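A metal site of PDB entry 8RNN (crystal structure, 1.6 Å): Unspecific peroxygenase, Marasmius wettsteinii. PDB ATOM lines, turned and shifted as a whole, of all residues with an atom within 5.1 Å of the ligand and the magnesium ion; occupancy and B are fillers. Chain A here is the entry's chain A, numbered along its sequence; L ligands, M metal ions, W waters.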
ATOM      1  N   PRO A  20     -23.408 -22.991  12.810  1.00  0.00           N
ATOM      2  CA  PRO A  20     -22.337 -23.950  12.513  1.00  0.00           C
ATOM      3  C   PRO A  20     -21.537 -24.407  13.723  1.00  0.00           C
ATOM      4  O   PRO A  20     -20.637 -25.231  13.584  1.00  0.00           O
ATOM      5  CB  PRO A  20     -21.488 -23.107  11.546  1.00  0.00           C
ATOM      6  CG  PRO A  20     -21.573 -21.718  12.119  1.00  0.00           C
ATOM      7  CD  PRO A  20     -23.003 -21.595  12.585  1.00  0.00           C
ATOM      8  N   CYS A  21     -21.904 -23.885  14.911  1.00  0.00           N
ATOM      9  CA  CYS A  21     -21.174 -24.138  16.138  1.00  0.00           C
ATOM     10  C   CYS A  21     -21.939 -25.141  16.998  1.00  0.00           C
ATOM     11  O   CYS A  21     -22.986 -24.798  17.513  1.00  0.00           O
ATOM     12  CB  CYS A  21     -20.972 -22.861  16.925  1.00  0.00           C
ATOM     13  SG  CYS A  21     -20.138 -23.190  18.500  1.00  0.00           S
ATOM     14  N   PRO A  22     -21.422 -26.369  17.203  1.00  0.00           N
ATOM     15  CA  PRO A  22     -22.072 -27.332  18.097  1.00  0.00           C
ATOM     16  C   PRO A  22     -22.092 -26.863  19.545  1.00  0.00           C
ATOM     17  O   PRO A  22     -22.982 -27.243  20.323  1.00  0.00           O
ATOM     18  CB  PRO A  22     -21.233 -28.614  17.928  1.00  0.00           C
ATOM     19  CG  PRO A  22     -19.870 -28.089  17.533  1.00  0.00           C
ATOM     20  CD  PRO A  22     -20.187 -26.916  16.616  1.00  0.00           C
ATOM     21  N   GLY A  23     -21.115 -26.040  19.950  1.00  0.00           N
ATOM     22  CA  GLY A  23     -21.075 -25.556  21.330  1.00  0.00           C
ATOM     23  C   GLY A  23     -22.283 -24.691  21.637  1.00  0.00           C
ATOM     24  O   GLY A  23     -23.005 -24.930  22.627  1.00  0.00           O
ATOM     25  N   LEU A  24     -22.550 -23.680  20.821  1.00  0.00           N
ATOM     26  CA  LEU A  24     -23.672 -22.781  21.036  1.00  0.00           C
ATOM     27  C   LEU A  24     -24.991 -23.489  20.728  1.00  0.00           C
ATOM     28  O   LEU A  24     -25.995 -23.272  21.411  1.00  0.00           O
ATOM     29  CB  LEU A  24     -23.480 -21.537  20.173  1.00  0.00           C
ATOM     30  CG  LEU A  24     -22.269 -20.676  20.514  1.00  0.00           C
ATOM     31  CD1 LEU A  24     -22.271 -19.430  19.653  1.00  0.00           C
ATOM     32  CD2 LEU A  24     -22.223 -20.289  22.002  1.00  0.00           C
ATOM     33  N   ILE A  45     -24.139 -15.290  26.034  1.00  0.00           N
ATOM     34  CA  ILE A  45     -23.209 -16.350  25.680  1.00  0.00           C
ATOM     35  C   ILE A  45     -22.242 -16.638  26.847  1.00  0.00           C
ATOM     36  O   ILE A  45     -21.966 -17.773  27.176  1.00  0.00           O
ATOM     37  CB  ILE A  45     -22.456 -15.994  24.384  1.00  0.00           C
ATOM     38  CG1 ILE A  45     -23.404 -16.006  23.183  1.00  0.00           C
ATOM     39  CG2 ILE A  45     -21.267 -16.915  24.172  1.00  0.00           C
ATOM     40  CD1 ILE A  45     -22.828 -15.394  21.927  1.00  0.00           C
ATOM     41  N   TYR A  53     -20.782 -25.349  30.626  1.00  0.00           N
ATOM     42  CA  TYR A  53     -19.528 -25.992  30.286  1.00  0.00           C
ATOM     43  C   TYR A  53     -18.356 -25.590  31.194  1.00  0.00           C
ATOM     44  O   TYR A  53     -17.286 -26.205  31.109  1.00  0.00           O
ATOM     45  CB  TYR A  53     -19.107 -25.602  28.864  1.00  0.00           C
ATOM     46  CG  TYR A  53     -20.038 -25.938  27.725  1.00  0.00           C
ATOM     47  CD1 TYR A  53     -20.705 -27.156  27.650  1.00  0.00           C
ATOM     48  CD2 TYR A  53     -20.193 -25.069  26.654  1.00  0.00           C
ATOM     49  CE1 TYR A  53     -21.506 -27.476  26.570  1.00  0.00           C
ATOM     50  CE2 TYR A  53     -20.995 -25.376  25.562  1.00  0.00           C
ATOM     51  CZ  TYR A  53     -21.650 -26.589  25.518  1.00  0.00           C
ATOM     52  OH  TYR A  53     -22.453 -26.902  24.453  1.00  0.00           O
ATOM     53  N   VAL A  55     -16.849 -22.807  30.805  1.00  0.00           N
ATOM     54  CA  VAL A  55     -15.973 -22.009  29.959  1.00  0.00           C
ATOM     55  C   VAL A  55     -16.052 -20.566  30.435  1.00  0.00           C
ATOM     56  O   VAL A  55     -17.134 -20.036  30.659  1.00  0.00           O
ATOM     57  CB  VAL A  55     -16.313 -22.167  28.465  1.00  0.00           C
ATOM     58  CG1 VAL A  55     -15.478 -21.209  27.618  1.00  0.00           C
ATOM     59  CG2 VAL A  55     -16.116 -23.583  27.991  1.00  0.00           C
ATOM     60  N   ILE A  59     -12.379 -16.192  26.845  1.00  0.00           N
ATOM     61  CA  ILE A  59     -12.513 -16.669  25.471  1.00  0.00           C
ATOM     62  C   ILE A  59     -13.892 -16.302  24.914  1.00  0.00           C
ATOM     63  O   ILE A  59     -14.014 -16.010  23.714  1.00  0.00           O
ATOM     64  CB  ILE A  59     -12.212 -18.172  25.343  1.00  0.00           C
ATOM     65  CG1 ILE A  59     -12.231 -18.613  23.879  1.00  0.00           C
ATOM     66  CG2 ILE A  59     -13.172 -18.981  26.185  1.00  0.00           C
ATOM     67  CD1 ILE A  59     -11.648 -19.973  23.626  1.00  0.00           C
ATOM     68  N   LEU A  60     -14.947 -16.314  25.745  1.00  0.00           N
ATOM     69  CA  LEU A  60     -16.296 -16.089  25.242  1.00  0.00           C
ATOM     70  C   LEU A  60     -16.549 -14.622  24.883  1.00  0.00           C
ATOM     71  O   LEU A  60     -17.293 -14.345  23.945  1.00  0.00           O
ATOM     72  CB  LEU A  60     -17.322 -16.623  26.241  1.00  0.00           C
ATOM     73  CG  LEU A  60     -17.270 -18.130  26.468  1.00  0.00           C
ATOM     74  CD1 LEU A  60     -18.285 -18.558  27.507  1.00  0.00           C
ATOM     75  CD2 LEU A  60     -17.499 -18.911  25.179  1.00  0.00           C
ATOM     76  N   ALA A  63     -14.380 -14.249  21.394  1.00  0.00           N
ATOM     77  CA  ALA A  63     -15.061 -14.876  20.280  1.00  0.00           C
ATOM     78  C   ALA A  63     -16.454 -14.278  20.061  1.00  0.00           C
ATOM     79  O   ALA A  63     -16.902 -14.088  18.922  1.00  0.00           O
ATOM     80  CB  ALA A  63     -15.155 -16.362  20.508  1.00  0.00           C
ATOM     81  N   GLY A  64     -17.155 -13.999  21.152  1.00  0.00           N
ATOM     82  CA  GLY A  64     -18.504 -13.483  21.089  1.00  0.00           C
ATOM     83  C   GLY A  64     -18.598 -12.168  20.321  1.00  0.00           C
ATOM     84  O   GLY A  64     -19.496 -11.972  19.505  1.00  0.00           O
ATOM     85  N   GLY A  67     -18.219 -12.729  16.762  1.00  0.00           N
ATOM     86  CA  GLY A  67     -19.458 -13.296  16.257  1.00  0.00           C
ATOM     87  C   GLY A  67     -20.566 -12.259  16.062  1.00  0.00           C
ATOM     88  O   GLY A  67     -21.375 -12.370  15.147  1.00  0.00           O
ATOM     89  N   LEU A  82     -24.025 -16.846  12.390  1.00  0.00           N
ATOM     90  CA  LEU A  82     -22.623 -17.206  12.528  1.00  0.00           C
ATOM     91  C   LEU A  82     -22.097 -18.016  11.342  1.00  0.00           C
ATOM     92  O   LEU A  82     -20.896 -18.263  11.268  1.00  0.00           O
ATOM     93  CB  LEU A  82     -22.448 -18.002  13.835  1.00  0.00           C
ATOM     94  CG  LEU A  82     -22.685 -17.218  15.133  1.00  0.00           C
ATOM     95  CD1 LEU A  82     -22.685 -18.158  16.328  1.00  0.00           C
ATOM     96  CD2 LEU A  82     -21.620 -16.144  15.316  1.00  0.00           C
ATOM     97  N   ILE A  88     -15.921 -15.854  11.367  1.00  0.00           N
ATOM     98  CA  ILE A  88     -15.364 -17.004  12.064  1.00  0.00           C
ATOM     99  C   ILE A  88     -15.465 -18.242  11.173  1.00  0.00           C
ATOM    100  O   ILE A  88     -14.517 -19.017  11.076  1.00  0.00           O
ATOM    101  CB  ILE A  88     -16.054 -17.221  13.424  1.00  0.00           C
ATOM    102  CG1 ILE A  88     -15.835 -16.023  14.339  1.00  0.00           C
ATOM    103  CG2 ILE A  88     -15.583 -18.518  14.077  1.00  0.00           C
ATOM    104  CD1 ILE A  88     -16.723 -16.023  15.577  1.00  0.00           C
ATOM    105  N   GLU A  89     -16.638 -18.440  10.546  1.00  0.00           N
ATOM    106  CA  GLU A  89     -16.863 -19.648   9.760  1.00  0.00           C
ATOM    107  C   GLU A  89     -15.774 -19.780   8.678  1.00  0.00           C
ATOM    108  O   GLU A  89     -15.404 -18.800   8.033  1.00  0.00           O
ATOM    109  CB  GLU A  89     -18.269 -19.658   9.163  1.00  0.00           C
ATOM    110  CG  GLU A  89     -18.675 -21.025   8.639  1.00  0.00           C
ATOM    111  CD  GLU A  89     -18.060 -21.405   7.303  1.00  0.00           C
ATOM    112  OE1 GLU A  89     -17.986 -20.515   6.418  1.00  0.00           O
ATOM    113  OE2 GLU A  89     -17.685 -22.578   7.139  1.00  0.00           O
ATOM    114  N   HIS A  90     -15.251 -21.002   8.550  1.00  0.00           N
ATOM    115  CA  HIS A  90     -14.078 -21.297   7.730  1.00  0.00           C
ATOM    116  C   HIS A  90     -14.219 -22.647   7.029  1.00  0.00           C
ATOM    117  O   HIS A  90     -15.015 -23.523   7.409  1.00  0.00           O
ATOM    118  CB  HIS A  90     -12.822 -21.326   8.626  1.00  0.00           C
ATOM    119  CG  HIS A  90     -12.971 -22.258   9.782  1.00  0.00           C
ATOM    120  ND1 HIS A  90     -12.915 -23.628   9.649  1.00  0.00           N
ATOM    121  CD2 HIS A  90     -13.216 -22.016  11.089  1.00  0.00           C
ATOM    122  CE1 HIS A  90     -13.141 -24.194  10.831  1.00  0.00           C
ATOM    123  NE2 HIS A  90     -13.325 -23.233  11.714  1.00  0.00           N
ATOM    124  N   ASP A  91     -13.375 -22.852   6.017  1.00  0.00           N
ATOM    125  CA  ASP A  91     -13.242 -24.130   5.356  1.00  0.00           C
ATOM    126  C   ASP A  91     -12.550 -25.152   6.254  1.00  0.00           C
ATOM    127  O   ASP A  91     -11.973 -24.791   7.287  1.00  0.00           O
ATOM    128  CB  ASP A  91     -12.441 -23.925   4.069  1.00  0.00           C
ATOM    129  CG  ASP A  91     -13.116 -22.996   3.090  1.00  0.00           C
ATOM    130  OD1 ASP A  91     -14.349 -22.917   3.109  1.00  0.00           O
ATOM    131  OD2 ASP A  91     -12.387 -22.355   2.297  1.00  0.00           O
ATOM    132  N   SER A  93     -13.846 -27.491   8.120  1.00  0.00           N
ATOM    133  CA  SER A  93     -14.556 -27.765   9.357  1.00  0.00           C
ATOM    134  C   SER A  93     -14.536 -29.266   9.628  1.00  0.00           C
ATOM    135  O   SER A  93     -14.306 -30.069   8.719  1.00  0.00           O
ATOM    136  CB  SER A  93     -15.969 -27.249   9.299  1.00  0.00           C
ATOM    137  OG  SER A  93     -16.015 -25.830   9.277  1.00  0.00           O
ATOM    138  N   LEU A  94     -14.819 -29.649  10.882  1.00  0.00           N
ATOM    139  CA  LEU A  94     -14.824 -31.040  11.338  1.00  0.00           C
ATOM    140  C   LEU A  94     -16.114 -31.769  10.960  1.00  0.00           C
ATOM    141  O   LEU A  94     -16.117 -33.005  10.923  1.00  0.00           O
ATOM    142  CB  LEU A  94     -14.662 -31.069  12.855  1.00  0.00           C
ATOM    143  CG  LEU A  94     -13.383 -30.445  13.411  1.00  0.00           C
ATOM    144  CD1 LEU A  94     -13.509 -30.168  14.912  1.00  0.00           C
ATOM    145  CD2 LEU A  94     -12.195 -31.314  13.110  1.00  0.00           C
ATOM    146  N   SER A  95     -17.206 -31.036  10.788  1.00  0.00           N
ATOM    147  CA  SER A  95     -18.519 -31.654  10.676  1.00  0.00           C
ATOM    148  C   SER A  95     -19.440 -30.924   9.688  1.00  0.00           C
ATOM    149  O   SER A  95     -20.598 -31.299   9.565  1.00  0.00           O
ATOM    150  CB  SER A  95     -19.167 -31.754  12.051  1.00  0.00           C
ATOM    151  OG  SER A  95     -19.575 -30.489  12.556  1.00  0.00           O
ATOM    152  N   ARG A  96     -18.919 -29.885   9.018  1.00  0.00           N
ATOM    153  CA  ARG A  96     -19.651 -29.116   8.022  1.00  0.00           C
ATOM    154  C   ARG A  96     -18.870 -29.137   6.717  1.00  0.00           C
ATOM    155  O   ARG A  96     -17.665 -29.350   6.725  1.00  0.00           O
ATOM    156  CB  ARG A  96     -19.858 -27.660   8.454  1.00  0.00           C
ATOM    157  CG  ARG A  96     -21.090 -27.356   9.289  1.00  0.00           C
ATOM    158  CD  ARG A  96     -21.187 -28.098  10.594  1.00  0.00           C
ATOM    159  NE  ARG A  96     -22.299 -27.602  11.390  1.00  0.00           N
ATOM    160  CZ  ARG A  96     -22.726 -28.145  12.529  1.00  0.00           C
ATOM    161  NH1 ARG A  96     -22.086 -29.155  13.080  1.00  0.00           N
ATOM    162  NH2 ARG A  96     -23.803 -27.644  13.102  1.00  0.00           N
ATOM    163  N   GLU A  97     -19.548 -28.840   5.597  1.00  0.00           N
ATOM    164  CA  GLU A  97     -18.899 -28.727   4.306  1.00  0.00           C
ATOM    165  C   GLU A  97     -18.392 -27.301   4.098  1.00  0.00           C
ATOM    166  O   GLU A  97     -18.866 -26.367   4.741  1.00  0.00           O
ATOM    167  CB  GLU A  97     -19.885 -29.099   3.200  1.00  0.00           C
ATOM    168  CG  GLU A  97     -20.400 -30.524   3.306  1.00  0.00           C
ATOM    169  CD  GLU A  97     -21.506 -30.917   2.352  1.00  0.00           C
ATOM    170  OE1 GLU A  97     -22.294 -30.039   1.925  1.00  0.00           O
ATOM    171  OE2 GLU A  97     -21.543 -32.124   1.993  1.00  0.00           O
ATOM    172  N   ASN A 104     -22.373 -25.106   4.651  1.00  0.00           N
ATOM    173  CA  ASN A 104     -21.426 -24.733   5.683  1.00  0.00           C
ATOM    174  C   ASN A 104     -22.109 -24.554   7.035  1.00  0.00           C
ATOM    175  O   ASN A 104     -21.463 -24.065   7.962  1.00  0.00           O
ATOM    176  CB  ASN A 104     -20.662 -23.451   5.318  1.00  0.00           C
ATOM    177  CG  ASN A 104     -21.478 -22.185   5.477  1.00  0.00           C
ATOM    178  OD1 ASN A 104     -22.694 -22.225   5.482  1.00  0.00           O
ATOM    179  ND2 ASN A 104     -20.819 -21.046   5.620  1.00  0.00           N
ATOM    180  N   GLU A 161     -11.152 -24.790  18.113  1.00  0.00           N
ATOM    181  CA  GLU A 161     -12.378 -25.570  18.081  1.00  0.00           C
ATOM    182  C   GLU A 161     -12.110 -27.020  18.510  1.00  0.00           C
ATOM    183  O   GLU A 161     -12.905 -27.612  19.233  1.00  0.00           O
ATOM    184  CB  GLU A 161     -13.024 -25.404  16.698  1.00  0.00           C
ATOM    185  CG  GLU A 161     -13.592 -24.016  16.530  1.00  0.00           C
ATOM    186  CD  GLU A 161     -13.819 -23.483  15.122  1.00  0.00           C
ATOM    187  OE1 GLU A 161     -13.466 -24.177  14.177  1.00  0.00           O
ATOM    188  OE2 GLU A 161     -14.360 -22.346  15.026  1.00  0.00           O
ATOM    189  N   PHE A 164     -11.714 -27.069  22.137  1.00  0.00           N
ATOM    190  CA  PHE A 164     -13.020 -26.991  22.785  1.00  0.00           C
ATOM    191  C   PHE A 164     -13.655 -28.386  22.910  1.00  0.00           C
ATOM    192  O   PHE A 164     -14.127 -28.727  24.000  1.00  0.00           O
ATOM    193  CB  PHE A 164     -13.971 -26.035  22.053  1.00  0.00           C
ATOM    194  CG  PHE A 164     -14.021 -24.620  22.582  1.00  0.00           C
ATOM    195  CD1 PHE A 164     -13.991 -24.383  23.947  1.00  0.00           C
ATOM    196  CD2 PHE A 164     -14.313 -23.562  21.725  1.00  0.00           C
ATOM    197  CE1 PHE A 164     -14.108 -23.096  24.444  1.00  0.00           C
ATOM    198  CE2 PHE A 164     -14.447 -22.269  22.238  1.00  0.00           C
ATOM    199  CZ  PHE A 164     -14.350 -22.042  23.595  1.00  0.00           C
ATOM    200  N   TYR A 165     -13.708 -29.192  21.838  1.00  0.00           N
ATOM    201  CA  TYR A 165     -14.372 -30.482  21.986  1.00  0.00           C
ATOM    202  C   TYR A 165     -13.601 -31.372  22.947  1.00  0.00           C
ATOM    203  O   TYR A 165     -14.222 -32.115  23.713  1.00  0.00           O
ATOM    204  CB  TYR A 165     -14.736 -31.134  20.644  1.00  0.00           C
ATOM    205  CG  TYR A 165     -13.660 -31.859  19.872  1.00  0.00           C
ATOM    206  CD1 TYR A 165     -13.129 -33.071  20.285  1.00  0.00           C
ATOM    207  CD2 TYR A 165     -13.237 -31.359  18.651  1.00  0.00           C
ATOM    208  CE1 TYR A 165     -12.176 -33.748  19.550  1.00  0.00           C
ATOM    209  CE2 TYR A 165     -12.278 -32.022  17.898  1.00  0.00           C
ATOM    210  CZ  TYR A 165     -11.750 -33.221  18.342  1.00  0.00           C
ATOM    211  OH  TYR A 165     -10.795 -33.858  17.610  1.00  0.00           O
ATOM    212  N   VAL A 168     -14.379 -29.449  26.780  1.00  0.00           N
ATOM    213  CA  VAL A 168     -15.725 -29.288  27.309  1.00  0.00           C
ATOM    214  C   VAL A 168     -16.409 -30.646  27.470  1.00  0.00           C
ATOM    215  O   VAL A 168     -17.220 -30.819  28.386  1.00  0.00           O
ATOM    216  CB  VAL A 168     -16.546 -28.320  26.430  1.00  0.00           C
ATOM    217  CG1 VAL A 168     -18.005 -28.314  26.803  1.00  0.00           C
ATOM    218  CG2 VAL A 168     -15.980 -26.911  26.467  1.00  0.00           C
ATOM    219  N   PHE A 187     -22.220 -34.950  21.222  1.00  0.00           N
ATOM    220  CA  PHE A 187     -22.102 -33.503  21.131  1.00  0.00           C
ATOM    221  C   PHE A 187     -22.276 -33.026  19.683  1.00  0.00           C
ATOM    222  O   PHE A 187     -23.067 -32.130  19.399  1.00  0.00           O
ATOM    223  CB  PHE A 187     -20.745 -33.115  21.728  1.00  0.00           C
ATOM    224  CG  PHE A 187     -20.388 -31.653  21.677  1.00  0.00           C
ATOM    225  CD1 PHE A 187     -21.094 -30.720  22.400  1.00  0.00           C
ATOM    226  CD2 PHE A 187     -19.325 -31.229  20.907  1.00  0.00           C
ATOM    227  CE1 PHE A 187     -20.744 -29.378  22.371  1.00  0.00           C
ATOM    228  CE2 PHE A 187     -18.981 -29.887  20.871  1.00  0.00           C
ATOM    229  CZ  PHE A 187     -19.701 -28.965  21.591  1.00  0.00           C
ATOM    230  N   PHE A 188     -21.529 -33.625  18.749  1.00  0.00           N
ATOM    231  CA  PHE A 188     -21.577 -33.253  17.338  1.00  0.00           C
ATOM    232  C   PHE A 188     -22.866 -33.748  16.667  1.00  0.00           C
ATOM    233  O   PHE A 188     -23.551 -32.995  15.996  1.00  0.00           O
ATOM    234  CB  PHE A 188     -20.350 -33.786  16.595  1.00  0.00           C
ATOM    235  CG  PHE A 188     -19.099 -32.939  16.665  1.00  0.00           C
ATOM    236  CD1 PHE A 188     -18.910 -31.889  15.784  1.00  0.00           C
ATOM    237  CD2 PHE A 188     -18.116 -33.195  17.615  1.00  0.00           C
ATOM    238  CE1 PHE A 188     -17.741 -31.123  15.840  1.00  0.00           C
ATOM    239  CE2 PHE A 188     -16.954 -32.429  17.663  1.00  0.00           C
ATOM    240  CZ  PHE A 188     -16.784 -31.389  16.772  1.00  0.00           C
HETATM  241  C1  LIG L   1     -17.328 -23.969  15.369  1.00  0.00           C
HETATM  242  C2  LIG L   1     -18.652 -19.598  16.842  1.00  0.00           C
HETATM  243  C3  LIG L   1     -18.290 -21.008  21.448  1.00  0.00           C
HETATM  244  C4  LIG L   1     -17.179 -25.438  19.962  1.00  0.00           C
HETATM  245  C5  LIG L   1     -17.766 -22.684  15.369  1.00  0.00           C
HETATM  246  C6  LIG L   1     -18.059 -21.919  14.211  1.00  0.00           C
HETATM  247  C7  LIG L   1     -18.450 -20.680  14.615  1.00  0.00           C
HETATM  248  C8  LIG L   1     -18.400 -20.683  16.048  1.00  0.00           C
HETATM  249  C9  LIG L   1     -18.887 -19.543  13.737  1.00  0.00           C
HETATM  250  C10 LIG L   1     -17.971 -22.437  12.790  1.00  0.00           C
HETATM  251  C11 LIG L   1     -16.495 -22.552  12.363  1.00  0.00           C
HETATM  252  C12 LIG L   1     -16.378 -23.558  11.278  1.00  0.00           C
HETATM  253  O1  LIG L   1     -16.297 -24.763  11.563  1.00  0.00           O
HETATM  254  O2  LIG L   1     -16.398 -23.178  10.074  1.00  0.00           O
HETATM  255  C13 LIG L   1     -18.588 -19.580  18.236  1.00  0.00           C
HETATM  256  C14 LIG L   1     -18.822 -18.401  18.995  1.00  0.00           C
HETATM  257  C15 LIG L   1     -18.755 -18.809  20.303  1.00  0.00           C
HETATM  258  C16 LIG L   1     -18.435 -20.235  20.303  1.00  0.00           C
HETATM  259  C17 LIG L   1     -19.150 -17.021  18.519  1.00  0.00           C
HETATM  260  C18 LIG L   1     -18.801 -17.876  21.438  1.00  0.00           C
HETATM  261  C19 LIG L   1     -17.861 -17.988  22.319  1.00  0.00           C
HETATM  262  C20 LIG L   1     -18.046 -22.354  21.457  1.00  0.00           C
HETATM  263  C21 LIG L   1     -18.007 -23.180  22.586  1.00  0.00           C
HETATM  264  C22 LIG L   1     -17.672 -24.430  22.191  1.00  0.00           C
HETATM  265  C23 LIG L   1     -17.524 -24.407  20.755  1.00  0.00           C
HETATM  266  C24 LIG L   1     -18.263 -22.751  24.017  1.00  0.00           C
HETATM  267  C25 LIG L   1     -17.625 -25.564  23.132  1.00  0.00           C
HETATM  268  C26 LIG L   1     -18.061 -26.703  22.726  1.00  0.00           C
HETATM  269  C27 LIG L   1     -17.083 -25.370  18.563  1.00  0.00           C
HETATM  270  C28 LIG L   1     -16.600 -26.522  17.753  1.00  0.00           C
HETATM  271  C29 LIG L   1     -16.663 -26.099  16.470  1.00  0.00           C
HETATM  272  C30 LIG L   1     -17.132 -24.710  16.537  1.00  0.00           C
HETATM  273  C31 LIG L   1     -16.165 -27.900  18.240  1.00  0.00           C
HETATM  274  C32 LIG L   1     -16.242 -26.832  15.197  1.00  0.00           C
HETATM  275  C33 LIG L   1     -17.380 -27.356  14.342  1.00  0.00           C
HETATM  276  C34 LIG L   1     -16.815 -27.988  13.083  1.00  0.00           C
HETATM  277  O3  LIG L   1     -17.544 -28.719  12.387  1.00  0.00           O
HETATM  278  O4  LIG L   1     -15.606 -27.805  12.769  1.00  0.00           O
HETATM  279  N1  LIG L   1     -17.965 -21.886  16.496  1.00  0.00           N
HETATM  280  N2  LIG L   1     -18.350 -20.630  19.020  1.00  0.00           N
HETATM  281  N3  LIG L   1     -17.769 -23.112  20.384  1.00  0.00           N
HETATM  282  N4  LIG L   1     -17.369 -24.293  17.813  1.00  0.00           N
HETATM  283 FE1  LIG L   1     -17.956 -22.563  18.393  1.00  0.00          FE
HETATM  284 MG    MG M   1     -16.876 -24.143   8.218  1.00  0.00          MG
HETATM  285  O   HOH W   1     -18.837 -24.533   9.005  1.00  0.00           O
HETATM  286  O   HOH W   2     -17.053 -25.427   6.543  1.00  0.00           O
HETATM  287  O   HOH W   3     -19.000 -25.760  11.378  1.00  0.00           O
HETATM  288  O   HOH W   4     -13.169 -26.649  12.998  1.00  0.00           O
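Of the 30 residues printed, 3 come within 4 Å of the magnesium ion.
The nearest printed residue that does not touch the magnesium ion is Asp 91 (4.3 Å).
The magnesium ion is bound by the side-chain carboxylate (OE2) of Glu 89 (2.1 Å), water W2 (2.1 Å), the backbone carbonyl oxygen (O) of His 90 (2.1 Å), an oxygen (O2) of the ligand (2.1 Å), water W1 (2.1 Å) and the side-chain hydroxyl (OG) of Ser 93 (2.2 Å).
The side-chain hydroxyl of Tyr 53 is in hydrogen-bond range of the backbone carbonyl oxygen of Gly 23 (2.7 Å).
OE1 of Glu 89 sits at hydrogen-bond distance from ND2 of Asn 104 (3.0 Å).
A ring nitrogen (NE2) of His 90 sits at hydrogen-bond distance from the side-chain carboxylate of Glu 161 (2.6 Å).
N of Leu 24 lies close to SG of Cys 21 (3.4 Å).
The side-chain sulfur of Cys 21 lies close to the backbone NH of Gly 23 (3.3 Å).
OG of Ser 95 is in hydrogen-bond range of NH1 of Arg 96, at 2.9 Å.
Water W4 bridges an oxygen (O4) of the ligand and the side-chain carboxylate of Glu 161.
Water W3 bridges the backbone carbonyl oxygen of Pro 20 (2.8 Å) and an oxygen (O1) of the ligand (2.9 Å).
Merely in contact with the ligand: Phe 187 (3.0 Å), Leu 60 (3.0 Å), Glu 161 (3.4 Å), Leu 82 (3.4 Å), Phe 164 (3.5 Å), Ile 88 (3.5 Å), Gly 23 (3.5 Å), Pro 22 (3.6 Å), Leu 24 (3.6 Å), Ala 63 (3.6 Å), Pro 20 (3.7 Å), Ile 45 (3.8 Å), Arg 96 (3.8 Å), Phe 188 (3.8 Å) and Val 168 (3.96 Å).
Hydrophobic or aromatic side chains within 4 Å of the ligand: Pro 20, Pro 22, Leu 24, Ile 45, Leu 60, Ala 63, Leu 82, Ile 88, His 90, Leu 94, Phe 164, Val 168, Phe 187 and Phe 188.
21 residues have an atom within 4 Å of the ligand: Pro 20, Cys 21, Pro 22, Gly 23, Leu 24, Ile 45, Leu 60, Ala 63, Leu 82, Ile 88, Glu 89, His 90, Ser 93, Leu 94, Ser 95, Arg 96, Glu 161, Phe 164, Val 168, Phe 187 and Phe 188.
Along chain A the residues within 4 Å of the ligand span positions 20 to 188.
The side-chain hydroxyl of Ser 95 is in hydrogen-bond range of an oxygen (O3) of the ligand, 2.7 Å away.
The backbone NH (N) of His 90 sits close to an oxygen (O2) of the ligand (2.9 Å).
An oxygen (O3) of the ligand sits at hydrogen-bond distance from the backbone NH of Ser 95 (2.8 Å).
NE2 of His 90 lies close to O1 of the ligand (3.3 Å).
N of Leu 94 sits at hydrogen-bond distance from O4 of the ligand.
An iron atom (FE1) of the ligand is bound by the side-chain sulfur (SG) of Cys 21 (2.3 Å).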
